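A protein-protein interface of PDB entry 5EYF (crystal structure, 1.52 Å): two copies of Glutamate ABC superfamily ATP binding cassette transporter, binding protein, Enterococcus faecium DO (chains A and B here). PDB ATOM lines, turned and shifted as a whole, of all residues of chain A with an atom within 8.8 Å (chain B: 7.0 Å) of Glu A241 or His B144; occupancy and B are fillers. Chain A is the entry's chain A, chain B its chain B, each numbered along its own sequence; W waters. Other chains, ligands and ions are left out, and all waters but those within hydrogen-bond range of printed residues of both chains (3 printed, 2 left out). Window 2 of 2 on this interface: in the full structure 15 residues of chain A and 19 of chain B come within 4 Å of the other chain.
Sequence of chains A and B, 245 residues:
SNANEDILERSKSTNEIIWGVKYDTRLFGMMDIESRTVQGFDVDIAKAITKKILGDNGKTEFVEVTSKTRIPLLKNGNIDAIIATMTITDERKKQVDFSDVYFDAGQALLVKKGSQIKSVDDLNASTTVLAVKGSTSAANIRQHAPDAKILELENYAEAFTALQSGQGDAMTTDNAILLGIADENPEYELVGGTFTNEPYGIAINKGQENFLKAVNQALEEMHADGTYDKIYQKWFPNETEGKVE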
ATOM      1  N   PHE A 103      -6.942  -2.737  18.239  1.00  0.00           N
ATOM      2  CA  PHE A 103      -7.824  -1.567  18.121  1.00  0.00           C
ATOM      3  C   PHE A 103      -8.615  -1.681  16.817  1.00  0.00           C
ATOM      4  O   PHE A 103      -8.031  -2.037  15.798  1.00  0.00           O
ATOM      5  CB  PHE A 103      -7.003  -0.253  18.126  1.00  0.00           C
ATOM      6  CG  PHE A 103      -7.847   1.013  18.197  1.00  0.00           C
ATOM      7  CD1 PHE A 103      -8.136   1.584  19.419  1.00  0.00           C
ATOM      8  CD2 PHE A 103      -8.341   1.604  17.034  1.00  0.00           C
ATOM      9  CE1 PHE A 103      -8.921   2.719  19.488  1.00  0.00           C
ATOM     10  CE2 PHE A 103      -9.141   2.754  17.097  1.00  0.00           C
ATOM     11  CZ  PHE A 103      -9.429   3.304  18.322  1.00  0.00           C
ATOM     12  N   ASP A 104      -9.920  -1.302  16.822  1.00  0.00           N
ATOM     13  CA  ASP A 104     -10.754  -1.396  15.620  1.00  0.00           C
ATOM     14  C   ASP A 104     -11.143  -0.003  15.123  1.00  0.00           C
ATOM     15  O   ASP A 104     -12.128   0.590  15.584  1.00  0.00           O
ATOM     16  CB  ASP A 104     -12.035  -2.221  15.882  1.00  0.00           C
ATOM     17  CG  ASP A 104     -11.794  -3.708  15.872  1.00  0.00           C
ATOM     18  OD1 ASP A 104     -11.114  -4.205  14.956  1.00  0.00           O
ATOM     19  OD2 ASP A 104     -12.390  -4.414  16.722  1.00  0.00           O
ATOM     20  N   ALA A 105     -10.375   0.514  14.182  1.00  0.00           N
ATOM     21  CA  ALA A 105     -10.661   1.808  13.554  1.00  0.00           C
ATOM     22  C   ALA A 105     -11.457   1.629  12.261  1.00  0.00           C
ATOM     23  O   ALA A 105     -11.786   0.504  11.859  1.00  0.00           O
ATOM     24  CB  ALA A 105      -9.353   2.562  13.303  1.00  0.00           C
ATOM     25  N   GLY A 106     -11.767   2.744  11.593  1.00  0.00           N
ATOM     26  CA  GLY A 106     -12.386   2.709  10.277  1.00  0.00           C
ATOM     27  C   GLY A 106     -12.203   4.043   9.595  1.00  0.00           C
ATOM     28  O   GLY A 106     -12.126   5.073  10.258  1.00  0.00           O
ATOM     29  N   ASN A 175     -10.903   7.110  11.560  1.00  0.00           N
ATOM     30  CA  ASN A 175     -11.741   7.858  12.494  1.00  0.00           C
ATOM     31  C   ASN A 175     -10.991   8.260  13.755  1.00  0.00           C
ATOM     32  O   ASN A 175     -11.079   9.419  14.180  1.00  0.00           O
ATOM     33  CB  ASN A 175     -13.034   7.077  12.831  1.00  0.00           C
ATOM     34  CG  ASN A 175     -12.804   5.677  13.423  1.00  0.00           C
ATOM     35  OD1 ASN A 175     -11.709   5.124  13.434  1.00  0.00           O
ATOM     36  ND2 ASN A 175     -13.893   5.098  13.918  1.00  0.00           N
ATOM     37  N   ALA A 176     -10.215   7.339  14.353  1.00  0.00           N
ATOM     38  CA  ALA A 176      -9.630   7.636  15.655  1.00  0.00           C
ATOM     39  C   ALA A 176      -8.502   8.648  15.522  1.00  0.00           C
ATOM     40  O   ALA A 176      -8.259   9.435  16.447  1.00  0.00           O
ATOM     41  CB  ALA A 176      -9.120   6.347  16.306  1.00  0.00           C
ATOM     42  N   GLY A 193     -20.023   8.249  10.287  1.00  0.00           N
ATOM     43  CA  GLY A 193     -19.571   6.876  10.559  1.00  0.00           C
ATOM     44  C   GLY A 193     -18.284   6.520   9.827  1.00  0.00           C
ATOM     45  O   GLY A 193     -17.444   7.377   9.522  1.00  0.00           O
ATOM     46  N   THR A 194     -18.130   5.237   9.513  1.00  0.00           N
ATOM     47  CA  THR A 194     -16.922   4.767   8.839  1.00  0.00           C
ATOM     48  C   THR A 194     -17.287   4.009   7.577  1.00  0.00           C
ATOM     49  O   THR A 194     -18.367   3.427   7.491  1.00  0.00           O
ATOM     50  CB  THR A 194     -16.053   3.857   9.741  1.00  0.00           C
ATOM     51  OG1 THR A 194     -16.825   2.715  10.162  1.00  0.00           O
ATOM     52  CG2 THR A 194     -15.598   4.578  10.958  1.00  0.00           C
ATOM     53  N   TYR A 228      -5.201  -3.781  29.413  1.00  0.00           N
ATOM     54  CA  TYR A 228      -5.697  -3.269  28.142  1.00  0.00           C
ATOM     55  C   TYR A 228      -6.858  -2.303  28.357  1.00  0.00           C
ATOM     56  O   TYR A 228      -6.883  -1.204  27.787  1.00  0.00           O
ATOM     57  CB  TYR A 228      -6.122  -4.425  27.239  1.00  0.00           C
ATOM     58  CG  TYR A 228      -6.741  -3.943  25.945  1.00  0.00           C
ATOM     59  CD1 TYR A 228      -5.943  -3.611  24.842  1.00  0.00           C
ATOM     60  CD2 TYR A 228      -8.134  -3.799  25.817  1.00  0.00           C
ATOM     61  CE1 TYR A 228      -6.514  -3.170  23.658  1.00  0.00           C
ATOM     62  CE2 TYR A 228      -8.680  -3.331  24.665  1.00  0.00           C
ATOM     63  CZ  TYR A 228      -7.885  -3.022  23.568  1.00  0.00           C
ATOM     64  OH  TYR A 228      -8.453  -2.552  22.395  1.00  0.00           O
ATOM     65  N   TYR A 232      -7.020   1.632  27.227  1.00  0.00           N
ATOM     66  CA  TYR A 232      -8.065   2.078  26.310  1.00  0.00           C
ATOM     67  C   TYR A 232      -8.869   3.217  26.933  1.00  0.00           C
ATOM     68  O   TYR A 232      -9.121   4.244  26.289  1.00  0.00           O
ATOM     69  CB  TYR A 232      -8.985   0.902  25.922  1.00  0.00           C
ATOM     70  CG  TYR A 232      -9.929   1.352  24.844  1.00  0.00           C
ATOM     71  CD1 TYR A 232      -9.619   1.150  23.491  1.00  0.00           C
ATOM     72  CD2 TYR A 232     -11.108   2.055  25.160  1.00  0.00           C
ATOM     73  CE1 TYR A 232     -10.469   1.596  22.481  1.00  0.00           C
ATOM     74  CE2 TYR A 232     -11.929   2.535  24.158  1.00  0.00           C
ATOM     75  CZ  TYR A 232     -11.580   2.322  22.821  1.00  0.00           C
ATOM     76  OH  TYR A 232     -12.416   2.793  21.849  1.00  0.00           O
ATOM     77  N   PHE A 236      -9.364   6.851  25.154  1.00  0.00           N
ATOM     78  CA  PHE A 236     -10.655   6.952  24.452  1.00  0.00           C
ATOM     79  C   PHE A 236     -11.782   6.917  25.469  1.00  0.00           C
ATOM     80  O   PHE A 236     -12.682   6.062  25.407  1.00  0.00           O
ATOM     81  CB  PHE A 236     -10.815   5.858  23.390  1.00  0.00           C
ATOM     82  CG  PHE A 236      -9.640   5.794  22.470  1.00  0.00           C
ATOM     83  CD1 PHE A 236      -9.502   6.726  21.461  1.00  0.00           C
ATOM     84  CD2 PHE A 236      -8.616   4.895  22.693  1.00  0.00           C
ATOM     85  CE1 PHE A 236      -8.351   6.727  20.645  1.00  0.00           C
ATOM     86  CE2 PHE A 236      -7.480   4.870  21.882  1.00  0.00           C
ATOM     87  CZ  PHE A 236      -7.333   5.795  20.865  1.00  0.00           C
ATOM     88  N   ASN A 238     -14.490   8.480  25.970  1.00  0.00           N
ATOM     89  CA  ASN A 238     -15.869   8.727  25.585  1.00  0.00           C
ATOM     90  C   ASN A 238     -16.277   7.992  24.330  1.00  0.00           C
ATOM     91  O   ASN A 238     -17.373   8.247  23.813  1.00  0.00           O
ATOM     92  CB  ASN A 238     -16.084  10.224  25.411  1.00  0.00           C
ATOM     93  CG  ASN A 238     -16.037  10.940  26.729  1.00  0.00           C
ATOM     94  OD1 ASN A 238     -16.817  10.629  27.619  1.00  0.00           O
ATOM     95  ND2 ASN A 238     -15.072  11.831  26.898  1.00  0.00           N
ATOM     96  N   GLU A 239     -15.419   7.123  23.796  1.00  0.00           N
ATOM     97  CA  GLU A 239     -15.718   6.407  22.560  1.00  0.00           C
ATOM     98  C   GLU A 239     -15.279   4.970  22.738  1.00  0.00           C
ATOM     99  O   GLU A 239     -14.080   4.674  22.745  1.00  0.00           O
ATOM    100  CB  GLU A 239     -15.029   7.021  21.344  1.00  0.00           C
ATOM    101  CG  GLU A 239     -15.604   6.484  20.021  1.00  0.00           C
ATOM    102  CD  GLU A 239     -17.104   6.206  20.094  1.00  0.00           C
ATOM    103  OE1 GLU A 239     -17.491   5.030  20.295  1.00  0.00           O
ATOM    104  OE2 GLU A 239     -17.897   7.170  19.965  1.00  0.00           O
ATOM    105  N   THR A 240     -16.244   4.081  22.856  1.00  0.00           N
ATOM    106  CA  THR A 240     -15.933   2.693  23.119  1.00  0.00           C
ATOM    107  C   THR A 240     -15.843   1.836  21.869  1.00  0.00           C
ATOM    108  O   THR A 240     -15.389   0.703  22.002  1.00  0.00           O
ATOM    109  CB  THR A 240     -16.960   2.075  24.051  1.00  0.00           C
ATOM    110  OG1 THR A 240     -18.245   2.208  23.437  1.00  0.00           O
ATOM    111  CG2 THR A 240     -16.952   2.764  25.393  1.00  0.00           C
ATOM    112  N   GLU A 241     -16.240   2.330  20.667  1.00  0.00           N
ATOM    113  CA  GLU A 241     -16.374   1.439  19.495  1.00  0.00           C
ATOM    114  C   GLU A 241     -15.049   0.796  19.080  1.00  0.00           C
ATOM    115  O   GLU A 241     -15.032  -0.324  18.553  1.00  0.00           O
ATOM    116  CB  GLU A 241     -16.927   2.189  18.266  1.00  0.00           C
ATOM    117  CG  GLU A 241     -18.448   2.145  17.950  1.00  0.00           C
ATOM    118  CD  GLU A 241     -19.258   0.975  18.503  1.00  0.00           C
ATOM    119  OE1 GLU A 241     -20.128   1.269  19.354  1.00  0.00           O
ATOM    120  OE2 GLU A 241     -19.123  -0.197  18.060  1.00  0.00           O
ATOM    121  N   GLY A 242     -13.945   1.475  19.294  1.00  0.00           N
ATOM    122  CA  GLY A 242     -12.654   0.949  18.863  1.00  0.00           C
ATOM    123  C   GLY A 242     -12.087  -0.133  19.756  1.00  0.00           C
ATOM    124  O   GLY A 242     -11.138  -0.817  19.371  1.00  0.00           O
ATOM    125  N   LYS A 243     -12.679  -0.344  20.921  1.00  0.00           N
ATOM    126  CA  LYS A 243     -12.138  -1.296  21.869  1.00  0.00           C
ATOM    127  C   LYS A 243     -12.331  -2.727  21.389  1.00  0.00           C
ATOM    128  O   LYS A 243     -13.424  -3.112  20.944  1.00  0.00           O
ATOM    129  CB  LYS A 243     -12.814  -1.099  23.227  1.00  0.00           C
ATOM    130  CG  LYS A 243     -12.223  -1.921  24.362  1.00  0.00           C
ATOM    131  CD  LYS A 243     -12.945  -1.640  25.674  1.00  0.00           C
ATOM    132  CE  LYS A 243     -12.427  -2.582  26.766  1.00  0.00           C
ATOM    133  NZ  LYS A 243     -13.030  -2.235  28.069  1.00  0.00           N
ATOM    134  N   VAL A 244     -11.267  -3.519  21.525  1.00  0.00           N
ATOM    135  CA  VAL A 244     -11.326  -4.960  21.302  1.00  0.00           C
ATOM    136  C   VAL A 244     -11.847  -5.592  22.589  1.00  0.00           C
ATOM    137  O   VAL A 244     -11.200  -5.521  23.645  1.00  0.00           O
ATOM    138  CB  VAL A 244      -9.950  -5.516  20.899  1.00  0.00           C
ATOM    139  CG1 VAL A 244      -9.961  -7.037  20.812  1.00  0.00           C
ATOM    140  CG2 VAL A 244      -9.518  -4.877  19.574  1.00  0.00           C
ATOM    141  N   GLU A 245     -13.051  -6.160  22.507  1.00  0.00           N
ATOM    142  CA  GLU A 245     -13.623  -6.988  23.533  1.00  0.00           C
ATOM    143  C   GLU A 245     -13.568  -8.465  23.067  1.00  0.00           C
ATOM    144  O   GLU A 245     -13.460  -9.391  23.868  1.00  0.00           O
ATOM    145  CB  GLU A 245     -15.088  -6.550  23.831  1.00  0.00           C
ATOM    146  CG  GLU A 245     -15.200  -5.074  24.274  1.00  0.00           C
ATOM    147  CD  GLU A 245     -16.609  -4.628  24.693  1.00  0.00           C
ATOM    148  OE1 GLU A 245     -17.619  -5.250  24.287  1.00  0.00           O
ATOM    149  OE2 GLU A 245     -16.716  -3.613  25.417  1.00  0.00           O
ATOM    150  OXT GLU A 245     -13.626  -8.797  21.865  1.00  0.00           O
ATOM    151  N   GLN B 107     -22.879  -1.940  12.196  1.00  0.00           N
ATOM    152  CA  GLN B 107     -24.286  -1.595  12.007  1.00  0.00           C
ATOM    153  C   GLN B 107     -24.457  -0.516  10.946  1.00  0.00           C
ATOM    154  O   GLN B 107     -23.648   0.404  10.837  1.00  0.00           O
ATOM    155  CB  GLN B 107     -24.908  -1.155  13.326  1.00  0.00           C
ATOM    156  CG  GLN B 107     -26.436  -1.080  13.244  1.00  0.00           C
ATOM    157  CD  GLN B 107     -27.067  -0.979  14.609  1.00  0.00           C
ATOM    158  OE1 GLN B 107     -26.468  -1.379  15.590  1.00  0.00           O
ATOM    159  NE2 GLN B 107     -28.264  -0.408  14.682  1.00  0.00           N
ATOM    160  N   VAL B 120     -26.654   7.790   9.805  1.00  0.00           N
ATOM    161  CA  VAL B 120     -27.227   7.778  11.137  1.00  0.00           C
ATOM    162  C   VAL B 120     -27.434   9.198  11.648  1.00  0.00           C
ATOM    163  O   VAL B 120     -28.316   9.428  12.470  1.00  0.00           O
ATOM    164  CB  VAL B 120     -26.320   6.932  12.056  1.00  0.00           C
ATOM    165  CG1 VAL B 120     -25.016   7.665  12.335  1.00  0.00           C
ATOM    166  CG2 VAL B 120     -27.059   6.510  13.330  1.00  0.00           C
ATOM    167  N   ASP B 121     -26.674  10.167  11.138  1.00  0.00           N
ATOM    168  CA  ASP B 121     -26.810  11.539  11.607  1.00  0.00           C
ATOM    169  C   ASP B 121     -28.154  12.153  11.214  1.00  0.00           C
ATOM    170  O   ASP B 121     -28.570  13.152  11.807  1.00  0.00           O
ATOM    171  CB  ASP B 121     -25.653  12.405  11.068  1.00  0.00           C
ATOM    172  CG  ASP B 121     -24.291  12.036  11.674  1.00  0.00           C
ATOM    173  OD1 ASP B 121     -24.274  11.392  12.742  1.00  0.00           O
ATOM    174  OD2 ASP B 121     -23.230  12.421  11.098  1.00  0.00           O
ATOM    175  N   LEU B 123     -31.114  10.636  11.479  1.00  0.00           N
ATOM    176  CA  LEU B 123     -32.204  10.076  12.257  1.00  0.00           C
ATOM    177  C   LEU B 123     -32.508  10.985  13.440  1.00  0.00           C
ATOM    178  O   LEU B 123     -31.595  11.505  14.098  1.00  0.00           O
ATOM    179  CB  LEU B 123     -31.842   8.674  12.736  1.00  0.00           C
ATOM    180  CG  LEU B 123     -31.550   7.693  11.594  1.00  0.00           C
ATOM    181  CD1 LEU B 123     -31.150   6.309  12.144  1.00  0.00           C
ATOM    182  CD2 LEU B 123     -32.761   7.571  10.654  1.00  0.00           C
ATOM    183  N   ALA B 139     -30.904  -1.204  20.454  1.00  0.00           N
ATOM    184  CA  ALA B 139     -30.173  -0.505  21.503  1.00  0.00           C
ATOM    185  C   ALA B 139     -29.095   0.409  20.923  1.00  0.00           C
ATOM    186  O   ALA B 139     -28.926   1.534  21.394  1.00  0.00           O
ATOM    187  CB  ALA B 139     -29.574  -1.508  22.492  1.00  0.00           C
ATOM    188  N   ASN B 140     -28.359  -0.047  19.900  1.00  0.00           N
ATOM    189  CA  ASN B 140     -27.338   0.817  19.309  1.00  0.00           C
ATOM    190  C   ASN B 140     -27.949   2.053  18.659  1.00  0.00           C
ATOM    191  O   ASN B 140     -27.327   3.129  18.656  1.00  0.00           O
ATOM    192  CB  ASN B 140     -26.509   0.059  18.272  1.00  0.00           C
ATOM    193  CG  ASN B 140     -25.527  -0.937  18.898  1.00  0.00           C
ATOM    194  OD1 ASN B 140     -25.181  -0.832  20.079  1.00  0.00           O
ATOM    195  ND2 ASN B 140     -25.081  -1.919  18.091  1.00  0.00           N
ATOM    196  N   ILE B 141     -29.136   1.923  18.064  1.00  0.00           N
ATOM    197  CA  ILE B 141     -29.778   3.111  17.509  1.00  0.00           C
ATOM    198  C   ILE B 141     -30.106   4.093  18.614  1.00  0.00           C
ATOM    199  O   ILE B 141     -29.907   5.305  18.468  1.00  0.00           O
ATOM    200  CB  ILE B 141     -31.047   2.762  16.718  1.00  0.00           C
ATOM    201  CG1 ILE B 141     -30.693   2.292  15.330  1.00  0.00           C
ATOM    202  CG2 ILE B 141     -31.880   4.034  16.552  1.00  0.00           C
ATOM    203  CD1 ILE B 141     -30.166   3.380  14.439  1.00  0.00           C
ATOM    204  N   ARG B 142     -30.645   3.597  19.727  1.00  0.00           N
ATOM    205  CA  ARG B 142     -31.036   4.514  20.785  1.00  0.00           C
ATOM    206  C   ARG B 142     -29.837   5.291  21.306  1.00  0.00           C
ATOM    207  O   ARG B 142     -29.998   6.379  21.859  1.00  0.00           O
ATOM    208  CB  ARG B 142     -31.748   3.745  21.904  1.00  0.00           C
ATOM    209  CG  ARG B 142     -33.043   3.096  21.409  1.00  0.00           C
ATOM    210  CD  ARG B 142     -33.904   2.450  22.496  1.00  0.00           C
ATOM    211  NE  ARG B 142     -35.235   2.098  21.980  1.00  0.00           N
ATOM    212  CZ  ARG B 142     -35.620   0.864  21.663  1.00  0.00           C
ATOM    213  NH1 ARG B 142     -34.779  -0.150  21.827  1.00  0.00           N
ATOM    214  NH2 ARG B 142     -36.846   0.635  21.192  1.00  0.00           N
ATOM    215  N   GLN B 143     -28.632   4.780  21.102  1.00  0.00           N
ATOM    216  CA  GLN B 143     -27.432   5.513  21.463  1.00  0.00           C
ATOM    217  C   GLN B 143     -26.966   6.461  20.363  1.00  0.00           C
ATOM    218  O   GLN B 143     -26.709   7.644  20.619  1.00  0.00           O
ATOM    219  CB  GLN B 143     -26.323   4.526  21.808  1.00  0.00           C
ATOM    220  CG  GLN B 143     -24.975   5.181  22.032  1.00  0.00           C
ATOM    221  CD  GLN B 143     -23.955   4.195  22.536  1.00  0.00           C
ATOM    222  OE1 GLN B 143     -24.307   3.212  23.169  1.00  0.00           O
ATOM    223  NE2 GLN B 143     -22.687   4.442  22.246  1.00  0.00           N
ATOM    224  N   HIS B 144     -26.862   5.962  19.130  1.00  0.00           N
ATOM    225  CA  HIS B 144     -26.292   6.769  18.059  1.00  0.00           C
ATOM    226  C   HIS B 144     -27.317   7.689  17.409  1.00  0.00           C
ATOM    227  O   HIS B 144     -26.930   8.617  16.697  1.00  0.00           O
ATOM    228  CB  HIS B 144     -25.647   5.847  17.017  1.00  0.00           C
ATOM    229  CG  HIS B 144     -24.387   5.200  17.502  1.00  0.00           C
ATOM    230  ND1 HIS B 144     -24.358   3.933  18.047  1.00  0.00           N
ATOM    231  CD2 HIS B 144     -23.118   5.668  17.569  1.00  0.00           C
ATOM    232  CE1 HIS B 144     -23.119   3.635  18.398  1.00  0.00           C
ATOM    233  NE2 HIS B 144     -22.350   4.677  18.133  1.00  0.00           N
ATOM    234  N   ALA B 145     -28.605   7.444  17.643  1.00  0.00           N
ATOM    235  CA  ALA B 145     -29.694   8.283  17.145  1.00  0.00           C
ATOM    236  C   ALA B 145     -30.729   8.402  18.256  1.00  0.00           C
ATOM    237  O   ALA B 145     -31.859   7.920  18.137  1.00  0.00           O
ATOM    238  CB  ALA B 145     -30.302   7.694  15.873  1.00  0.00           C
ATOM    239  N   PRO B 146     -30.360   9.044  19.367  1.00  0.00           N
ATOM    240  CA  PRO B 146     -31.177   8.943  20.588  1.00  0.00           C
ATOM    241  C   PRO B 146     -32.567   9.533  20.461  1.00  0.00           C
ATOM    242  O   PRO B 146     -33.442   9.186  21.262  1.00  0.00           O
ATOM    243  CB  PRO B 146     -30.341   9.702  21.627  1.00  0.00           C
ATOM    244  CG  PRO B 146     -29.537  10.660  20.829  1.00  0.00           C
ATOM    245  CD  PRO B 146     -29.208   9.942  19.547  1.00  0.00           C
ATOM    246  N   ASP B 147     -32.802  10.408  19.489  1.00  0.00           N
ATOM    247  CA  ASP B 147     -34.112  11.003  19.277  1.00  0.00           C
ATOM    248  C   ASP B 147     -34.978  10.194  18.328  1.00  0.00           C
ATOM    249  O   ASP B 147     -36.179  10.456  18.228  1.00  0.00           O
ATOM    250  CB  ASP B 147     -33.960  12.422  18.719  1.00  0.00           C
ATOM    251  CG  ASP B 147     -33.270  13.352  19.681  1.00  0.00           C
ATOM    252  OD1 ASP B 147     -33.467  13.193  20.907  1.00  0.00           O
ATOM    253  OD2 ASP B 147     -32.527  14.239  19.211  1.00  0.00           O
ATOM    254  N   PHE B 195     -21.843   2.594  11.639  1.00  0.00           N
ATOM    255  CA  PHE B 195     -21.682   3.444  12.812  1.00  0.00           C
ATOM    256  C   PHE B 195     -21.418   2.640  14.081  1.00  0.00           C
ATOM    257  O   PHE B 195     -21.366   3.221  15.175  1.00  0.00           O
ATOM    258  CB  PHE B 195     -22.888   4.399  12.990  1.00  0.00           C
ATOM    259  CG  PHE B 195     -24.240   3.720  13.036  1.00  0.00           C
ATOM    260  CD1 PHE B 195     -24.793   3.320  14.249  1.00  0.00           C
ATOM    261  CD2 PHE B 195     -24.953   3.490  11.866  1.00  0.00           C
ATOM    262  CE1 PHE B 195     -26.066   2.684  14.281  1.00  0.00           C
ATOM    263  CE2 PHE B 195     -26.208   2.873  11.888  1.00  0.00           C
ATOM    264  CZ  PHE B 195     -26.758   2.463  13.085  1.00  0.00           C
ATOM    265  N   THR B 196     -21.223   1.327  13.957  1.00  0.00           N
ATOM    266  CA  THR B 196     -20.662   0.526  15.032  1.00  0.00           C
ATOM    267  C   THR B 196     -19.656  -0.447  14.441  1.00  0.00           C
ATOM    268  O   THR B 196     -19.601  -0.656  13.222  1.00  0.00           O
ATOM    269  CB  THR B 196     -21.705  -0.302  15.774  1.00  0.00           C
ATOM    270  OG1 THR B 196     -22.152  -1.361  14.915  1.00  0.00           O
ATOM    271  CG2 THR B 196     -22.900   0.550  16.230  1.00  0.00           C
ATOM    272  N   ASN B 197     -18.881  -1.087  15.316  1.00  0.00           N
ATOM    273  CA  ASN B 197     -18.164  -2.299  14.931  1.00  0.00           C
ATOM    274  C   ASN B 197     -18.905  -3.498  15.496  1.00  0.00           C
ATOM    275  O   ASN B 197     -19.310  -3.480  16.657  1.00  0.00           O
ATOM    276  CB  ASN B 197     -16.730  -2.258  15.451  1.00  0.00           C
ATOM    277  CG  ASN B 197     -15.951  -1.152  14.818  1.00  0.00           C
ATOM    278  OD1 ASN B 197     -16.138  -0.851  13.633  1.00  0.00           O
ATOM    279  ND2 ASN B 197     -15.100  -0.515  15.594  1.00  0.00           N
ATOM    280  N   GLU B 198     -19.097  -4.532  14.675  1.00  0.00           N
ATOM    281  CA  GLU B 198     -19.817  -5.742  15.087  1.00  0.00           C
ATOM    282  C   GLU B 198     -18.945  -6.937  14.754  1.00  0.00           C
ATOM    283  O   GLU B 198     -19.169  -7.611  13.745  1.00  0.00           O
ATOM    284  CB  GLU B 198     -21.177  -5.858  14.386  1.00  0.00           C
ATOM    285  CG  GLU B 198     -22.123  -4.662  14.589  1.00  0.00           C
ATOM    286  CD  GLU B 198     -22.696  -4.534  15.983  1.00  0.00           C
ATOM    287  OE1 GLU B 198     -22.919  -5.533  16.674  1.00  0.00           O
ATOM    288  OE2 GLU B 198     -22.961  -3.395  16.415  1.00  0.00           O
ATOM    289  N   PRO B 199     -17.928  -7.216  15.569  1.00  0.00           N
ATOM    290  CA  PRO B 199     -17.091  -8.410  15.324  1.00  0.00           C
ATOM    291  C   PRO B 199     -17.836  -9.679  15.722  1.00  0.00           C
ATOM    292  O   PRO B 199     -18.283  -9.809  16.866  1.00  0.00           O
ATOM    293  CB  PRO B 199     -15.869  -8.183  16.218  1.00  0.00           C
ATOM    294  CG  PRO B 199     -16.394  -7.277  17.312  1.00  0.00           C
ATOM    295  CD  PRO B 199     -17.443  -6.406  16.705  1.00  0.00           C
HETATM  296  O   HOH W   1     -21.694  -1.953  18.805  1.00  0.00           O
HETATM  297  O   HOH W   2     -17.363  -2.014  19.164  1.00  0.00           O
HETATM  298  O   HOH W   3     -13.841   2.681  15.538  1.00  0.00           O
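Among the printed residues, merely in contact across the chains: Glu A241 with Thr B196 (3.5 Å) and Glu A241 with His B144 (3.9 Å).
The side-chain carboxylate (OE2) of Glu A241 is in hydrogen-bond range of the backbone NH (N) of Asn B197 (2.9 Å).
The side-chain amide nitrogen (ND2) of Asn B197 lies within hydrogen-bond range of the backbone carbonyl oxygen (O) of Asp A104 (3.2 Å).
Water W3 lies within hydrogen-bond range of the backbone carbonyl oxygen of Asp A104 (2.7 Å), the side-chain amide nitrogen of Asn A175 (2.9 Å) and the side-chain amide nitrogen of Asn B197 (3.4 Å).
Water W2 lies within hydrogen-bond range of the side-chain carboxylate (OE2) of Glu A241 (2.8 Å) and the backbone carbonyl oxygen (O) of Asn B197 (3.5 Å).
Water W1 lies within hydrogen-bond range of the side-chain carboxylate (OE2) of Glu B198, the side-chain carboxylate (OE2) of Glu A241 and the side-chain amide nitrogen (ND2) of Asn B140.
Printed residues of chain B within 4 Å of Asp A104: Asn B197.
Ala A176 touches none of the printed residues of chain B.
Glu A241 touches just these residues of chain B: His B144 (3.9 Å), Thr B196 (3.5 Å) and Asn B197 (2.9 Å).
Gly A242 touches none of the printed residues of chain B.
His B144 touches just one residue of chain A: Glu A241.
Printed residues of chain A within 4 Å of Thr B196: Glu A241.
Of the printed residues of chain A, Asn B197 touches Asp A104 and Glu A241.
The nearest printed residue of chain A that does not touch His B144 is Glu A239 (5.3 Å).
The nearest printed residue of chain B that does not touch Asp A104 is Pro B199 (5.0 Å).
No position is printed for both chains.
The side-chain hydroxyl (OG1) of Thr B196 sits at hydrogen-bond distance from the side-chain carboxylate (OE2) of Glu B198 (2.7 Å).
OE1 of Glu A239 lies within hydrogen-bond range of N of Glu A241 (3.0 Å).
O of Gly A242 is in hydrogen-bond range of N of Asp A104.
NE2 of His B144 lies within hydrogen-bond range of O of Phe B195, 3.4 Å away.
The backbone NH (N) of Gln B107 lies within hydrogen-bond range of the side-chain hydroxyl (OG1) of Thr B196 (2.9 Å).
A ring nitrogen (ND1) of His B144 is in hydrogen-bond range of the backbone carbonyl oxygen of Asn B140 (3.1 Å).
Along chain A the printed residues that touch a printed residue of chain B span positions 104 to 241.
Of the 18 printed residues of chain B, 3 touch a printed residue of chain A.
Hydrophobic or aromatic side chains of chain B that line the printed part of chain A: His B144.
Among the printed residues, 4 pairs touch across the chains.
Among the printed residues, no Asp or Glu carboxylate lies within 4 Å of a Lys or Arg side-chain nitrogen of the other chain.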
